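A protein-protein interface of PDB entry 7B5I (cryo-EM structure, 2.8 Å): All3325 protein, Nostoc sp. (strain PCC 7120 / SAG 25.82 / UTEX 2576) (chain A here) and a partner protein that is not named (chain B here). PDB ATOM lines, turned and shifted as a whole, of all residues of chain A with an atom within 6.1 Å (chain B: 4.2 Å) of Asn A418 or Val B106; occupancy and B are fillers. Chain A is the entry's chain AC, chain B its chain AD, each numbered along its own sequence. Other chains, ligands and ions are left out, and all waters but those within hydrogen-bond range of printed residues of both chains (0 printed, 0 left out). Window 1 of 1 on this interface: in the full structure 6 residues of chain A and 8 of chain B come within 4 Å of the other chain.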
ATOM      1  N   LYS A 413      14.391   3.497 -11.700  1.00  0.00           N
ATOM      2  CA  LYS A 413      14.996   4.532 -12.526  1.00  0.00           C
ATOM      3  C   LYS A 413      14.959   5.880 -11.826  1.00  0.00           C
ATOM      4  O   LYS A 413      15.932   6.642 -11.879  1.00  0.00           O
ATOM      5  CB  LYS A 413      14.278   4.606 -13.869  1.00  0.00           C
ATOM      6  CG  LYS A 413      14.859   5.625 -14.818  1.00  0.00           C
ATOM      7  CD  LYS A 413      14.217   5.517 -16.178  1.00  0.00           C
ATOM      8  CE  LYS A 413      14.729   6.595 -17.106  1.00  0.00           C
ATOM      9  NZ  LYS A 413      14.151   6.446 -18.462  1.00  0.00           N
ATOM     10  N   ALA A 414      13.844   6.188 -11.157  1.00  0.00           N
ATOM     11  CA  ALA A 414      13.745   7.450 -10.434  1.00  0.00           C
ATOM     12  C   ALA A 414      14.815   7.555  -9.358  1.00  0.00           C
ATOM     13  O   ALA A 414      15.491   8.586  -9.239  1.00  0.00           O
ATOM     14  CB  ALA A 414      12.356   7.591  -9.818  1.00  0.00           C
ATOM     15  N   MET A 415      14.989   6.494  -8.569  1.00  0.00           N
ATOM     16  CA  MET A 415      16.004   6.524  -7.517  1.00  0.00           C
ATOM     17  C   MET A 415      17.398   6.769  -8.094  1.00  0.00           C
ATOM     18  O   MET A 415      18.146   7.640  -7.610  1.00  0.00           O
ATOM     19  CB  MET A 415      15.958   5.220  -6.723  1.00  0.00           C
ATOM     20  CG  MET A 415      17.016   5.074  -5.645  1.00  0.00           C
ATOM     21  SD  MET A 415      18.534   4.300  -6.217  1.00  0.00           S
ATOM     22  CE  MET A 415      17.913   2.676  -6.610  1.00  0.00           C
ATOM     23  N   ILE A 416      17.753   6.030  -9.148  1.00  0.00           N
ATOM     24  CA  ILE A 416      19.096   6.155  -9.712  1.00  0.00           C
ATOM     25  C   ILE A 416      19.317   7.562 -10.260  1.00  0.00           C
ATOM     26  O   ILE A 416      20.382   8.167 -10.064  1.00  0.00           O
ATOM     27  CB  ILE A 416      19.328   5.080 -10.788  1.00  0.00           C
ATOM     28  CG1 ILE A 416      19.309   3.690 -10.167  1.00  0.00           C
ATOM     29  CG2 ILE A 416      20.648   5.299 -11.489  1.00  0.00           C
ATOM     30  CD1 ILE A 416      19.240   2.585 -11.186  1.00  0.00           C
ATOM     31  N   GLU A 417      18.318   8.109 -10.952  1.00  0.00           N
ATOM     32  CA  GLU A 417      18.490   9.430 -11.544  1.00  0.00           C
ATOM     33  C   GLU A 417      18.603  10.516 -10.484  1.00  0.00           C
ATOM     34  O   GLU A 417      19.355  11.481 -10.658  1.00  0.00           O
ATOM     35  CB  GLU A 417      17.349   9.738 -12.505  1.00  0.00           C
ATOM     36  CG  GLU A 417      17.483   9.049 -13.843  1.00  0.00           C
ATOM     37  CD  GLU A 417      16.417   9.475 -14.816  1.00  0.00           C
ATOM     38  OE1 GLU A 417      15.411  10.060 -14.371  1.00  0.00           O
ATOM     39  OE2 GLU A 417      16.579   9.229 -16.026  1.00  0.00           O
ATOM     40  N   ASN A 418      17.870  10.389  -9.379  1.00  0.00           N
ATOM     41  CA  ASN A 418      18.009  11.387  -8.323  1.00  0.00           C
ATOM     42  C   ASN A 418      19.406  11.356  -7.711  1.00  0.00           C
ATOM     43  O   ASN A 418      20.010  12.412  -7.458  1.00  0.00           O
ATOM     44  CB  ASN A 418      16.942  11.173  -7.254  1.00  0.00           C
ATOM     45  CG  ASN A 418      15.572  11.599  -7.715  1.00  0.00           C
ATOM     46  OD1 ASN A 418      15.440  12.390  -8.642  1.00  0.00           O
ATOM     47  ND2 ASN A 418      14.541  11.087  -7.067  1.00  0.00           N
ATOM     48  N   PHE A 419      19.947  10.155  -7.487  1.00  0.00           N
ATOM     49  CA  PHE A 419      21.309  10.061  -6.967  1.00  0.00           C
ATOM     50  C   PHE A 419      22.320  10.684  -7.931  1.00  0.00           C
ATOM     51  O   PHE A 419      23.209  11.446  -7.525  1.00  0.00           O
ATOM     52  CB  PHE A 419      21.651   8.601  -6.684  1.00  0.00           C
ATOM     53  CG  PHE A 419      23.081   8.376  -6.302  1.00  0.00           C
ATOM     54  CD1 PHE A 419      23.542   8.757  -5.065  1.00  0.00           C
ATOM     55  CD2 PHE A 419      23.957   7.755  -7.172  1.00  0.00           C
ATOM     56  CE1 PHE A 419      24.851   8.547  -4.706  1.00  0.00           C
ATOM     57  CE2 PHE A 419      25.267   7.542  -6.813  1.00  0.00           C
ATOM     58  CZ  PHE A 419      25.714   7.939  -5.581  1.00  0.00           C
ATOM     59  N   LEU A 420      22.198  10.371  -9.220  1.00  0.00           N
ATOM     60  CA  LEU A 420      23.143  10.922 -10.185  1.00  0.00           C
ATOM     61  C   LEU A 420      23.010  12.434 -10.323  1.00  0.00           C
ATOM     62  O   LEU A 420      24.008  13.118 -10.562  1.00  0.00           O
ATOM     63  CB  LEU A 420      22.971  10.248 -11.538  1.00  0.00           C
ATOM     64  CG  LEU A 420      23.432   8.796 -11.575  1.00  0.00           C
ATOM     65  CD1 LEU A 420      23.073   8.167 -12.895  1.00  0.00           C
ATOM     66  CD2 LEU A 420      24.912   8.741 -11.341  1.00  0.00           C
ATOM     67  N   THR A 421      21.797  12.974 -10.187  1.00  0.00           N
ATOM     68  CA  THR A 421      21.624  14.424 -10.216  1.00  0.00           C
ATOM     69  C   THR A 421      22.330  15.086  -9.041  1.00  0.00           C
ATOM     70  O   THR A 421      22.995  16.122  -9.200  1.00  0.00           O
ATOM     71  CB  THR A 421      20.139  14.767 -10.194  1.00  0.00           C
ATOM     72  OG1 THR A 421      19.488  14.133 -11.296  1.00  0.00           O
ATOM     73  CG2 THR A 421      19.938  16.260 -10.294  1.00  0.00           C
ATOM     74  N   LEU A 422      22.177  14.514  -7.844  1.00  0.00           N
ATOM     75  CA  LEU A 422      22.902  15.054  -6.700  1.00  0.00           C
ATOM     76  C   LEU A 422      24.402  14.991  -6.909  1.00  0.00           C
ATOM     77  O   LEU A 422      25.127  15.879  -6.453  1.00  0.00           O
ATOM     78  CB  LEU A 422      22.536  14.309  -5.423  1.00  0.00           C
ATOM     79  CG  LEU A 422      21.166  14.581  -4.827  1.00  0.00           C
ATOM     80  CD1 LEU A 422      20.924  13.606  -3.703  1.00  0.00           C
ATOM     81  CD2 LEU A 422      21.113  15.995  -4.323  1.00  0.00           C
ATOM     82  N   GLN A 423      24.894  13.946  -7.574  1.00  0.00           N
ATOM     83  CA  GLN A 423      26.331  13.883  -7.817  1.00  0.00           C
ATOM     84  C   GLN A 423      26.768  14.913  -8.848  1.00  0.00           C
ATOM     85  O   GLN A 423      27.848  15.499  -8.726  1.00  0.00           O
ATOM     86  CB  GLN A 423      26.742  12.481  -8.249  1.00  0.00           C
ATOM     87  CG  GLN A 423      26.604  11.472  -7.137  1.00  0.00           C
ATOM     88  CD  GLN A 423      27.367  11.891  -5.903  1.00  0.00           C
ATOM     89  OE1 GLN A 423      28.538  12.258  -5.975  1.00  0.00           O
ATOM     90  NE2 GLN A 423      26.708  11.837  -4.758  1.00  0.00           N
ATOM     91  N   ILE B  59       3.585  20.675  -2.421  1.00  0.00           N
ATOM     92  CA  ILE B  59       2.630  19.672  -2.877  1.00  0.00           C
ATOM     93  C   ILE B  59       1.754  19.251  -1.708  1.00  0.00           C
ATOM     94  O   ILE B  59       2.251  19.039  -0.598  1.00  0.00           O
ATOM     95  CB  ILE B  59       3.348  18.468  -3.503  1.00  0.00           C
ATOM     96  CG1 ILE B  59       4.145  18.931  -4.720  1.00  0.00           C
ATOM     97  CG2 ILE B  59       2.361  17.404  -3.897  1.00  0.00           C
ATOM     98  CD1 ILE B  59       5.023  17.877  -5.317  1.00  0.00           C
ATOM     99  N   ASP B  88      12.516  10.224  -1.988  1.00  0.00           N
ATOM    100  CA  ASP B  88      12.196  10.424  -3.395  1.00  0.00           C
ATOM    101  C   ASP B  88      10.720  10.123  -3.612  1.00  0.00           C
ATOM    102  O   ASP B  88      10.220   9.091  -3.162  1.00  0.00           O
ATOM    103  CB  ASP B  88      13.054   9.520  -4.278  1.00  0.00           C
ATOM    104  CG  ASP B  88      14.532   9.810  -4.149  1.00  0.00           C
ATOM    105  OD1 ASP B  88      14.893  10.983  -3.921  1.00  0.00           O
ATOM    106  OD2 ASP B  88      15.334   8.863  -4.271  1.00  0.00           O
ATOM    107  N   LEU B  89      10.004  11.041  -4.251  1.00  0.00           N
ATOM    108  CA  LEU B  89       8.574  10.848  -4.465  1.00  0.00           C
ATOM    109  C   LEU B  89       8.219  10.573  -5.918  1.00  0.00           C
ATOM    110  O   LEU B  89       8.735  11.222  -6.828  1.00  0.00           O
ATOM    111  CB  LEU B  89       7.792  12.062  -3.960  1.00  0.00           C
ATOM    112  CG  LEU B  89       7.911  12.375  -2.468  1.00  0.00           C
ATOM    113  CD1 LEU B  89       7.142  13.640  -2.121  1.00  0.00           C
ATOM    114  CD2 LEU B  89       7.420  11.201  -1.632  1.00  0.00           C
ATOM    115  N   TRP B 104       5.357  11.895 -12.569  1.00  0.00           N
ATOM    116  CA  TRP B 104       5.983  13.054 -11.950  1.00  0.00           C
ATOM    117  C   TRP B 104       7.005  12.560 -10.935  1.00  0.00           C
ATOM    118  O   TRP B 104       6.667  11.779 -10.036  1.00  0.00           O
ATOM    119  CB  TRP B 104       4.949  13.948 -11.265  1.00  0.00           C
ATOM    120  CG  TRP B 104       3.967  14.604 -12.190  1.00  0.00           C
ATOM    121  CD1 TRP B 104       4.094  15.820 -12.786  1.00  0.00           C
ATOM    122  CD2 TRP B 104       2.697  14.090 -12.598  1.00  0.00           C
ATOM    123  NE1 TRP B 104       2.990  16.092 -13.548  1.00  0.00           N
ATOM    124  CE2 TRP B 104       2.116  15.045 -13.449  1.00  0.00           C
ATOM    125  CE3 TRP B 104       1.995  12.913 -12.328  1.00  0.00           C
ATOM    126  CZ2 TRP B 104       0.869  14.859 -14.034  1.00  0.00           C
ATOM    127  CZ3 TRP B 104       0.761  12.733 -12.908  1.00  0.00           C
ATOM    128  CH2 TRP B 104       0.210  13.698 -13.751  1.00  0.00           C
ATOM    129  N   LYS B 105       8.250  13.003 -11.087  1.00  0.00           N
ATOM    130  CA  LYS B 105       9.337  12.632 -10.192  1.00  0.00           C
ATOM    131  C   LYS B 105       9.724  13.845  -9.366  1.00  0.00           C
ATOM    132  O   LYS B 105      10.074  14.891  -9.925  1.00  0.00           O
ATOM    133  CB  LYS B 105      10.542  12.119 -10.973  1.00  0.00           C
ATOM    134  CG  LYS B 105      10.224  10.950 -11.862  1.00  0.00           C
ATOM    135  CD  LYS B 105      11.435  10.509 -12.642  1.00  0.00           C
ATOM    136  CE  LYS B 105      11.089   9.365 -13.574  1.00  0.00           C
ATOM    137  NZ  LYS B 105      12.255   8.957 -14.394  1.00  0.00           N
ATOM    138  N   VAL B 106       9.643  13.706  -8.047  1.00  0.00           N
ATOM    139  CA  VAL B 106       9.988  14.779  -7.127  1.00  0.00           C
ATOM    140  C   VAL B 106      11.339  14.471  -6.494  1.00  0.00           C
ATOM    141  O   VAL B 106      11.666  13.309  -6.251  1.00  0.00           O
ATOM    142  CB  VAL B 106       8.924  14.934  -6.024  1.00  0.00           C
ATOM    143  CG1 VAL B 106       9.104  16.254  -5.289  1.00  0.00           C
ATOM    144  CG2 VAL B 106       7.528  14.846  -6.622  1.00  0.00           C
ATOM    145  N   ASN B 107      12.123  15.510  -6.227  1.00  0.00           N
ATOM    146  CA  ASN B 107      13.441  15.328  -5.635  1.00  0.00           C
ATOM    147  C   ASN B 107      13.571  15.955  -4.251  1.00  0.00           C
ATOM    148  O   ASN B 107      13.182  17.106  -4.041  1.00  0.00           O
ATOM    149  CB  ASN B 107      14.525  15.879  -6.565  1.00  0.00           C
ATOM    150  CG  ASN B 107      15.914  15.406  -6.185  1.00  0.00           C
ATOM    151  OD1 ASN B 107      16.071  14.463  -5.409  1.00  0.00           O
ATOM    152  ND2 ASN B 107      16.932  16.059  -6.734  1.00  0.00           N
ATOM    153  N   HIS B 135      10.153  20.350  -1.550  1.00  0.00           N
ATOM    154  CA  HIS B 135      11.055  19.533  -2.349  1.00  0.00           C
ATOM    155  C   HIS B 135      12.035  20.439  -3.078  1.00  0.00           C
ATOM    156  O   HIS B 135      11.843  21.654  -3.151  1.00  0.00           O
ATOM    157  CB  HIS B 135      10.270  18.683  -3.346  1.00  0.00           C
ATOM    158  CG  HIS B 135       9.473  19.485  -4.330  1.00  0.00           C
ATOM    159  ND1 HIS B 135       9.976  19.873  -5.552  1.00  0.00           N
ATOM    160  CD2 HIS B 135       8.210  19.965  -4.276  1.00  0.00           C
ATOM    161  CE1 HIS B 135       9.060  20.563  -6.204  1.00  0.00           C
ATOM    162  NE2 HIS B 135       7.979  20.634  -5.451  1.00  0.00           N
ATOM    163  N   GLY B 137      12.999  19.747  -6.517  1.00  0.00           N
ATOM    164  CA  GLY B 137      12.995  19.468  -7.939  1.00  0.00           C
ATOM    165  C   GLY B 137      11.770  18.688  -8.370  1.00  0.00           C
ATOM    166  O   GLY B 137      11.163  17.950  -7.594  1.00  0.00           O
ATOM    167  N   LEU B 138      11.459  18.816  -9.658  1.00  0.00           N
ATOM    168  CA  LEU B 138      10.303  18.154 -10.249  1.00  0.00           C
ATOM    169  C   LEU B 138      10.555  17.914 -11.730  1.00  0.00           C
ATOM    170  O   LEU B 138      11.118  18.768 -12.415  1.00  0.00           O
ATOM    171  CB  LEU B 138       9.033  18.984 -10.069  1.00  0.00           C
ATOM    172  CG  LEU B 138       7.745  18.435 -10.673  1.00  0.00           C
ATOM    173  CD1 LEU B 138       7.454  17.042 -10.173  1.00  0.00           C
ATOM    174  CD2 LEU B 138       6.606  19.366 -10.348  1.00  0.00           C
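The side-chain amide nitrogen (ND2) of Asn A418 sits at hydrogen-bond distance from the side-chain carboxylate (OD1) of Asp B88, 3.2 Å away. The side-chain carboxylate of Glu A417 lies within salt-bridge range of the side-chain amino group of Lys B105.
The backbone carbonyl oxygen (O) of Ala A414 lies close to the side-chain amide nitrogen (ND2) of Asn A418. The backbone carbonyl oxygen (O) of Leu B89 sits at hydrogen-bond distance from the backbone NH (N) of Val B106 (2.9 Å). The backbone carbonyl oxygen (O) of Glu A417 lies within hydrogen-bond range of the side-chain hydroxyl (OG1) of Thr A421 (2.7 Å). O of Gly B137 sits at hydrogen-bond distance from N of Asn B107, 3.0 Å away.
Among the printed residues, merely in contact across the chains: Asn A418 with Val B106 and Asn A418 with Asn B107.
Ala A414 touches none of the printed residues of chain B. Of the printed residues of chain B, Glu A417 touches Lys B105. Of chain B, only Asp B88 (3.2 Å), Val B106 (3.7 Å) and Asn B107 (3.7 Å) come within 4 Å of Asn A418. Printed residues of chain A within 4 Å of Asp B88: Asn A418 (3.2 Å). Printed residues of chain A within 4 Å of Lys B105: Glu A417. Val B106 touches just one residue of chain A: Asn A418 (3.7 Å). Of the printed residues of chain A, Asn B107 touches Asn A418. Leu B138 touches none of the printed residues of chain A. The nearest printed residue of chain B that does not touch Asn A418 is Leu B89 (5.3 Å). The nearest printed residue of chain A that does not touch Asp B88 is Met A415 (4.1 Å).
Printed residues of chain B that touch a printed residue of chain A: Asp B88, Lys B105, Val B106 and Asn B107. Along chain B the printed residues that touch a printed residue of chain A span positions 88 to 107. Among the printed residues, 4 pairs touch across the chains.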
